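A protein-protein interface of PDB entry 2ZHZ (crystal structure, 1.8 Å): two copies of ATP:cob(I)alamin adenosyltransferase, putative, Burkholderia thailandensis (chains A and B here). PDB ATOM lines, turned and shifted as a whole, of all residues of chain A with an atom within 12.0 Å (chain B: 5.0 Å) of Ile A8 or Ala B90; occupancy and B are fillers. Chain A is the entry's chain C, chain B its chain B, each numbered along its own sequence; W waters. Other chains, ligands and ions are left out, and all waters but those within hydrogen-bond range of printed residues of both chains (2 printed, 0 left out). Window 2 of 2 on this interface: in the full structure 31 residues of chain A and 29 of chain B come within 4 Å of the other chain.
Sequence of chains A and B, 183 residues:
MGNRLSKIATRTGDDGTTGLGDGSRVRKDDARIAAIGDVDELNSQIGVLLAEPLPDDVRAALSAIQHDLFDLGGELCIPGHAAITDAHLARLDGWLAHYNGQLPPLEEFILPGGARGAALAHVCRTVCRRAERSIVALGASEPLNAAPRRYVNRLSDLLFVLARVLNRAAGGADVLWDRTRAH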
ATOM      1  N   LEU A   5      11.456  28.484   5.232  1.00  0.00           N
ATOM      2  CA  LEU A   5      12.045  27.216   4.711  1.00  0.00           C
ATOM      3  C   LEU A   5      11.107  26.522   3.735  1.00  0.00           C
ATOM      4  O   LEU A   5       9.935  26.295   4.043  1.00  0.00           O
ATOM      5  CB  LEU A   5      12.351  26.251   5.858  1.00  0.00           C
ATOM      6  CG  LEU A   5      13.472  26.604   6.833  1.00  0.00           C
ATOM      7  CD1 LEU A   5      13.559  25.535   7.911  1.00  0.00           C
ATOM      8  CD2 LEU A   5      14.786  26.712   6.081  1.00  0.00           C
ATOM      9  N   SER A   6      11.626  26.183   2.558  1.00  0.00           N
ATOM     10  CA  SER A   6      10.825  25.492   1.556  1.00  0.00           C
ATOM     11  C   SER A   6      10.502  24.094   2.062  1.00  0.00           C
ATOM     12  O   SER A   6      11.317  23.470   2.740  1.00  0.00           O
ATOM     13  CB  SER A   6      11.586  25.385   0.232  1.00  0.00           C
ATOM     14  OG  SER A   6      10.890  24.553  -0.680  1.00  0.00           O
ATOM     15  N   LYS A   7       9.311  23.609   1.730  1.00  0.00           N
ATOM     16  CA  LYS A   7       8.876  22.280   2.148  1.00  0.00           C
ATOM     17  C   LYS A   7       9.274  21.239   1.108  1.00  0.00           C
ATOM     18  O   LYS A   7       9.006  20.048   1.273  1.00  0.00           O
ATOM     19  CB  LYS A   7       7.356  22.259   2.333  1.00  0.00           C
ATOM     20  CG  LYS A   7       6.845  23.200   3.414  1.00  0.00           C
ATOM     21  CD  LYS A   7       7.407  22.828   4.779  1.00  0.00           C
ATOM     22  CE  LYS A   7       6.996  21.415   5.183  1.00  0.00           C
ATOM     23  NZ  LYS A   7       7.593  21.007   6.488  1.00  0.00           N
ATOM     24  N   ILE A   8       9.915  21.696   0.036  1.00  0.00           N
ATOM     25  CA  ILE A   8      10.339  20.804  -1.037  1.00  0.00           C
ATOM     26  C   ILE A   8      11.806  20.419  -0.904  1.00  0.00           C
ATOM     27  O   ILE A   8      12.664  21.269  -0.658  1.00  0.00           O
ATOM     28  CB  ILE A   8      10.132  21.460  -2.421  1.00  0.00           C
ATOM     29  CG1 ILE A   8       8.692  21.968  -2.549  1.00  0.00           C
ATOM     30  CG2 ILE A   8      10.444  20.453  -3.527  1.00  0.00           C
ATOM     31  CD1 ILE A   8       7.633  20.889  -2.415  1.00  0.00           C
ATOM     32  N   ALA A   9      12.085  19.131  -1.072  1.00  0.00           N
ATOM     33  CA  ALA A   9      13.446  18.626  -0.976  1.00  0.00           C
ATOM     34  C   ALA A   9      14.336  19.368  -1.964  1.00  0.00           C
ATOM     35  O   ALA A   9      13.865  19.874  -2.982  1.00  0.00           O
ATOM     36  CB  ALA A   9      13.471  17.133  -1.273  1.00  0.00           C
ATOM     37  N   THR A  10      15.625  19.428  -1.664  1.00  0.00           N
ATOM     38  CA  THR A  10      16.558  20.120  -2.535  1.00  0.00           C
ATOM     39  C   THR A  10      17.325  19.152  -3.420  1.00  0.00           C
ATOM     40  O   THR A  10      17.668  18.045  -3.001  1.00  0.00           O
ATOM     41  CB  THR A  10      17.584  20.927  -1.723  1.00  0.00           C
ATOM     42  OG1 THR A  10      18.473  20.024  -1.057  1.00  0.00           O
ATOM     43  CG2 THR A  10      16.885  21.788  -0.686  1.00  0.00           C
ATOM     44  N   ARG A  11      17.575  19.577  -4.653  1.00  0.00           N
ATOM     45  CA  ARG A  11      18.343  18.788  -5.607  1.00  0.00           C
ATOM     46  C   ARG A  11      19.753  19.366  -5.512  1.00  0.00           C
ATOM     47  O   ARG A  11      19.925  20.521  -5.114  1.00  0.00           O
ATOM     48  CB  ARG A  11      17.781  18.961  -7.024  1.00  0.00           C
ATOM     49  CG  ARG A  11      16.399  18.353  -7.218  1.00  0.00           C
ATOM     50  CD  ARG A  11      15.751  18.818  -8.518  1.00  0.00           C
ATOM     51  NE  ARG A  11      16.524  18.429  -9.695  1.00  0.00           N
ATOM     52  CZ  ARG A  11      16.074  17.629 -10.658  1.00  0.00           C
ATOM     53  NH1 ARG A  11      14.844  17.125 -10.593  1.00  0.00           N
ATOM     54  NH2 ARG A  11      16.854  17.329 -11.687  1.00  0.00           N
ATOM     55  N   THR A  12      20.760  18.576  -5.865  1.00  0.00           N
ATOM     56  CA  THR A  12      22.140  19.037  -5.775  1.00  0.00           C
ATOM     57  C   THR A  12      22.424  20.281  -6.614  1.00  0.00           C
ATOM     58  O   THR A  12      23.331  21.051  -6.307  1.00  0.00           O
ATOM     59  CB  THR A  12      23.129  17.917  -6.170  1.00  0.00           C
ATOM     60  OG1 THR A  12      22.853  17.472  -7.502  1.00  0.00           O
ATOM     61  CG2 THR A  12      22.999  16.737  -5.212  1.00  0.00           C
ATOM     62  N   GLY A  13      21.638  20.488  -7.663  1.00  0.00           N
ATOM     63  CA  GLY A  13      21.849  21.651  -8.506  1.00  0.00           C
ATOM     64  C   GLY A  13      20.898  22.801  -8.227  1.00  0.00           C
ATOM     65  O   GLY A  13      20.895  23.796  -8.953  1.00  0.00           O
ATOM     66  N   ASP A  14      20.097  22.681  -7.171  1.00  0.00           N
ATOM     67  CA  ASP A  14      19.133  23.722  -6.831  1.00  0.00           C
ATOM     68  C   ASP A  14      19.747  25.052  -6.405  1.00  0.00           C
ATOM     69  O   ASP A  14      19.112  26.101  -6.538  1.00  0.00           O
ATOM     70  CB  ASP A  14      18.185  23.241  -5.726  1.00  0.00           C
ATOM     71  CG  ASP A  14      16.991  22.474  -6.268  1.00  0.00           C
ATOM     72  OD1 ASP A  14      16.752  22.516  -7.495  1.00  0.00           O
ATOM     73  OD2 ASP A  14      16.281  21.840  -5.458  1.00  0.00           O
ATOM     74  N   ASP A  15      20.970  25.018  -5.891  1.00  0.00           N
ATOM     75  CA  ASP A  15      21.614  26.246  -5.444  1.00  0.00           C
ATOM     76  C   ASP A  15      22.268  27.031  -6.578  1.00  0.00           C
ATOM     77  O   ASP A  15      22.933  28.040  -6.343  1.00  0.00           O
ATOM     78  CB  ASP A  15      22.640  25.937  -4.347  1.00  0.00           C
ATOM     79  CG  ASP A  15      23.796  25.092  -4.840  1.00  0.00           C
ATOM     80  OD1 ASP A  15      23.749  24.612  -5.995  1.00  0.00           O
ATOM     81  OD2 ASP A  15      24.753  24.901  -4.062  1.00  0.00           O
ATOM     82  N   ASP B  86       6.219  26.574  -3.642  1.00  0.00           N
ATOM     83  CA  ASP B  86       6.522  25.161  -3.444  1.00  0.00           C
ATOM     84  C   ASP B  86       5.507  24.321  -4.202  1.00  0.00           C
ATOM     85  O   ASP B  86       5.816  23.225  -4.667  1.00  0.00           O
ATOM     86  CB  ASP B  86       6.474  24.787  -1.959  1.00  0.00           C
ATOM     87  CG  ASP B  86       7.697  25.250  -1.199  1.00  0.00           C
ATOM     88  OD1 ASP B  86       8.718  25.570  -1.841  1.00  0.00           O
ATOM     89  OD2 ASP B  86       7.644  25.278   0.050  1.00  0.00           O
ATOM     90  N   ALA B  87       4.293  24.843  -4.324  1.00  0.00           N
ATOM     91  CA  ALA B  87       3.230  24.143  -5.032  1.00  0.00           C
ATOM     92  C   ALA B  87       3.662  23.857  -6.468  1.00  0.00           C
ATOM     93  O   ALA B  87       3.421  22.773  -7.000  1.00  0.00           O
ATOM     94  CB  ALA B  87       1.962  24.985  -5.026  1.00  0.00           C
ATOM     95  N   HIS B  88       4.295  24.844  -7.094  1.00  0.00           N
ATOM     96  CA  HIS B  88       4.768  24.703  -8.467  1.00  0.00           C
ATOM     97  C   HIS B  88       5.852  23.632  -8.548  1.00  0.00           C
ATOM     98  O   HIS B  88       5.828  22.782  -9.432  1.00  0.00           O
ATOM     99  CB  HIS B  88       5.328  26.035  -8.973  1.00  0.00           C
ATOM    100  CG  HIS B  88       4.291  27.100  -9.139  1.00  0.00           C
ATOM    101  ND1 HIS B  88       3.435  27.141 -10.217  1.00  0.00           N
ATOM    102  CD2 HIS B  88       3.962  28.154  -8.357  1.00  0.00           C
ATOM    103  CE1 HIS B  88       2.623  28.176 -10.093  1.00  0.00           C
ATOM    104  NE2 HIS B  88       2.923  28.806  -8.972  1.00  0.00           N
ATOM    105  N   LEU B  89       6.798  23.682  -7.619  1.00  0.00           N
ATOM    106  CA  LEU B  89       7.886  22.718  -7.586  1.00  0.00           C
ATOM    107  C   LEU B  89       7.376  21.316  -7.262  1.00  0.00           C
ATOM    108  O   LEU B  89       7.882  20.321  -7.790  1.00  0.00           O
ATOM    109  CB  LEU B  89       8.927  23.136  -6.543  1.00  0.00           C
ATOM    110  CG  LEU B  89       9.541  24.526  -6.721  1.00  0.00           C
ATOM    111  CD1 LEU B  89      10.526  24.787  -5.592  1.00  0.00           C
ATOM    112  CD2 LEU B  89      10.238  24.617  -8.075  1.00  0.00           C
ATOM    113  N   ALA B  90       6.377  21.237  -6.387  1.00  0.00           N
ATOM    114  CA  ALA B  90       5.814  19.951  -6.000  1.00  0.00           C
ATOM    115  C   ALA B  90       5.138  19.295  -7.193  1.00  0.00           C
ATOM    116  O   ALA B  90       5.251  18.083  -7.389  1.00  0.00           O
ATOM    117  CB  ALA B  90       4.807  20.134  -4.865  1.00  0.00           C
ATOM    118  N   ARG B  91       4.442  20.096  -7.993  1.00  0.00           N
ATOM    119  CA  ARG B  91       3.756  19.556  -9.154  1.00  0.00           C
ATOM    120  C   ARG B  91       4.740  18.991 -10.177  1.00  0.00           C
ATOM    121  O   ARG B  91       4.480  17.951 -10.784  1.00  0.00           O
ATOM    122  CB  ARG B  91       2.871  20.616  -9.804  1.00  0.00           C
ATOM    123  CG  ARG B  91       2.013  20.042 -10.908  1.00  0.00           C
ATOM    124  CD  ARG B  91       0.849  20.943 -11.248  1.00  0.00           C
ATOM    125  NE  ARG B  91       1.277  22.232 -11.778  1.00  0.00           N
ATOM    126  CZ  ARG B  91       0.454  23.097 -12.356  1.00  0.00           C
ATOM    127  NH1 ARG B  91      -0.836  22.800 -12.471  1.00  0.00           N
ATOM    128  NH2 ARG B  91       0.915  24.249 -12.829  1.00  0.00           N
ATOM    129  N   LEU B  92       5.865  19.674 -10.371  1.00  0.00           N
ATOM    130  CA  LEU B  92       6.874  19.192 -11.308  1.00  0.00           C
ATOM    131  C   LEU B  92       7.456  17.890 -10.768  1.00  0.00           C
ATOM    132  O   LEU B  92       7.618  16.921 -11.509  1.00  0.00           O
ATOM    133  CB  LEU B  92       7.998  20.216 -11.482  1.00  0.00           C
ATOM    134  CG  LEU B  92       7.701  21.541 -12.186  1.00  0.00           C
ATOM    135  CD1 LEU B  92       9.006  22.297 -12.353  1.00  0.00           C
ATOM    136  CD2 LEU B  92       7.057  21.305 -13.547  1.00  0.00           C
ATOM    137  N   ASP B  93       7.769  17.871  -9.475  1.00  0.00           N
ATOM    138  CA  ASP B  93       8.322  16.674  -8.847  1.00  0.00           C
ATOM    139  C   ASP B  93       7.339  15.516  -8.969  1.00  0.00           C
ATOM    140  O   ASP B  93       7.739  14.360  -9.090  1.00  0.00           O
ATOM    141  CB  ASP B  93       8.625  16.917  -7.365  1.00  0.00           C
ATOM    142  CG  ASP B  93       9.861  17.763  -7.149  1.00  0.00           C
ATOM    143  OD1 ASP B  93      10.640  17.938  -8.105  1.00  0.00           O
ATOM    144  OD2 ASP B  93      10.060  18.241  -6.010  1.00  0.00           O
ATOM    145  N   GLY B  94       6.050  15.838  -8.928  1.00  0.00           N
ATOM    146  CA  GLY B  94       5.022  14.818  -9.037  1.00  0.00           C
ATOM    147  C   GLY B  94       4.965  14.235 -10.434  1.00  0.00           C
ATOM    148  O   GLY B  94       4.873  13.019 -10.602  1.00  0.00           O
ATOM    149  N   ARG B 150      14.990  26.772  -9.075  1.00  0.00           N
ATOM    150  CA  ARG B 150      14.615  25.406  -8.731  1.00  0.00           C
ATOM    151  C   ARG B 150      13.560  24.864  -9.678  1.00  0.00           C
ATOM    152  O   ARG B 150      13.529  23.665  -9.963  1.00  0.00           O
ATOM    153  CB  ARG B 150      14.095  25.349  -7.295  1.00  0.00           C
ATOM    154  CG  ARG B 150      15.095  25.839  -6.265  1.00  0.00           C
ATOM    155  CD  ARG B 150      14.524  25.715  -4.859  1.00  0.00           C
ATOM    156  NE  ARG B 150      14.457  24.322  -4.418  1.00  0.00           N
ATOM    157  CZ  ARG B 150      13.698  23.891  -3.415  1.00  0.00           C
ATOM    158  NH1 ARG B 150      12.930  24.744  -2.747  1.00  0.00           N
ATOM    159  NH2 ARG B 150      13.714  22.611  -3.073  1.00  0.00           N
ATOM    160  N   ARG B 154      14.066  21.532 -12.359  1.00  0.00           N
ATOM    161  CA  ARG B 154      13.185  20.377 -12.437  1.00  0.00           C
ATOM    162  C   ARG B 154      12.556  20.222 -13.815  1.00  0.00           C
ATOM    163  O   ARG B 154      12.393  19.108 -14.302  1.00  0.00           O
ATOM    164  CB  ARG B 154      12.089  20.492 -11.373  1.00  0.00           C
ATOM    165  CG  ARG B 154      12.609  20.274  -9.969  1.00  0.00           C
ATOM    166  CD  ARG B 154      11.595  20.650  -8.893  1.00  0.00           C
ATOM    167  NE  ARG B 154      12.142  20.332  -7.578  1.00  0.00           N
ATOM    168  CZ  ARG B 154      13.241  20.884  -7.076  1.00  0.00           C
ATOM    169  NH1 ARG B 154      13.907  21.797  -7.771  1.00  0.00           N
ATOM    170  NH2 ARG B 154      13.704  20.494  -5.897  1.00  0.00           N
HETATM  171  O   HOH W   1      12.929  16.766  -8.307  1.00  0.00           O
HETATM  172  O   HOH W   2      12.551  18.088  -4.972  1.00  0.00           O
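O of Ala A9 sits at hydrogen-bond distance from NH2 of Arg B150, at 2.7 Å.
NH1 of Arg B150 is in hydrogen-bond range of OG of Ser A6, 2.9 Å away.
NH2 of Arg B154 lies within salt-bridge range of OD2 of Asp A14 (2.9 Å).
OD2 of Asp A14 is in salt-bridge range of NE of Arg B150, 3.3 Å away.
OG of Ser A6 lies within hydrogen-bond range of OD1 of Asp B86 (2.7 Å).
The guanidinium group of Arg B150 lies within hydrogen-bond range of the backbone carbonyl oxygen of Ile A8 (3.0 Å).
The side-chain carboxylate (OD2) of Asp B86 lies within hydrogen-bond range of the backbone NH (N) of Lys A7 (2.9 Å).
NH2 of Arg B154 lies within hydrogen-bond range of O of Ala A9 (3.0 Å).
NE of Arg B154 is in salt-bridge range of OD1 of Asp B93 (2.9 Å).
N of Arg A11 is in hydrogen-bond range of OD2 of Asp A14, at 2.7 Å.
The side-chain hydroxyl (OG) of Ser A6 lies within hydrogen-bond range of the backbone NH (N) of Ile A8 (3.1 Å).
The backbone carbonyl oxygen (O) of Arg B150 lies within hydrogen-bond range of the guanidinium group (NH1) of Arg B154, 2.9 Å away.
Among the printed residues, merely in contact across the chains: Ile A8 with Asp B93 (3.3 Å), Arg A11 with Arg B154 (3.6 Å), Ile A8 with Asp B86 (3.6 Å), Ile A8 with Ala B90 (3.8 Å) and Thr A10 with Arg B150 (3.8 Å).
Printed residues of chain B within 4 Å of Ser A6: Asp B86 (2.7 Å) and Arg B150 (2.9 Å).
Printed residues of chain B within 4 Å of Lys A7: Asp B86 (2.9 Å).
Printed residues of chain B within 4 Å of Ile A8: Asp B86 (3.6 Å), Ala B90 (3.8 Å), Asp B93 (3.3 Å) and Arg B150 (3.0 Å).
Printed residues of chain B within 4 Å of Arg A11: Arg B154 (3.6 Å).
Printed residues of chain B within 4 Å of Asp A14: Arg B150 (3.3 Å) and Arg B154 (2.9 Å).
Asp A15 touches none of the printed residues of chain B.
Asp B86 touches just these residues of chain A: Ser A6 (2.7 Å), Lys A7 (2.9 Å) and Ile A8 (3.6 Å).
Leu B89 touches none of the printed residues of chain A.
Of chain A, only Ile A8 (3.8 Å) comes within 4 Å of Ala B90.
No residue of chain A comes within 4 Å of Leu B92.
Asp B93 touches one residue of chain A.
The nearest residue of chain A that does not touch Ala B90 is Lys A7 (7.4 Å).
Of the 11 printed residues of chain B, 5 touch a printed residue of chain A.
Hydrophobic or aromatic side chains of chain B within 4 Å of the printed part of chain A: Ala B90.
Among the printed residues, 13 pairs touch across the chains.
Among the printed residues, Asp or Glu carboxylates within 4 Å of a Lys or Arg side-chain nitrogen of the other chain: Asp A14 with Arg B150 (3.3 Å) and Asp A14 with Arg B154 (2.9 Å).
No position is printed for both chains.
Of the 13 pairs that touch across the chains among the printed residues, none has its exchanged pair printed and touching as well.
Water W1 bridges OD1 of Asp B93 (2.6 Å) and NH1 of Arg A11 (3.0 Å).
Water W2 lies within hydrogen-bond range of OD2 of Asp B93, NH2 of Arg B154 and O of Ala A9.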
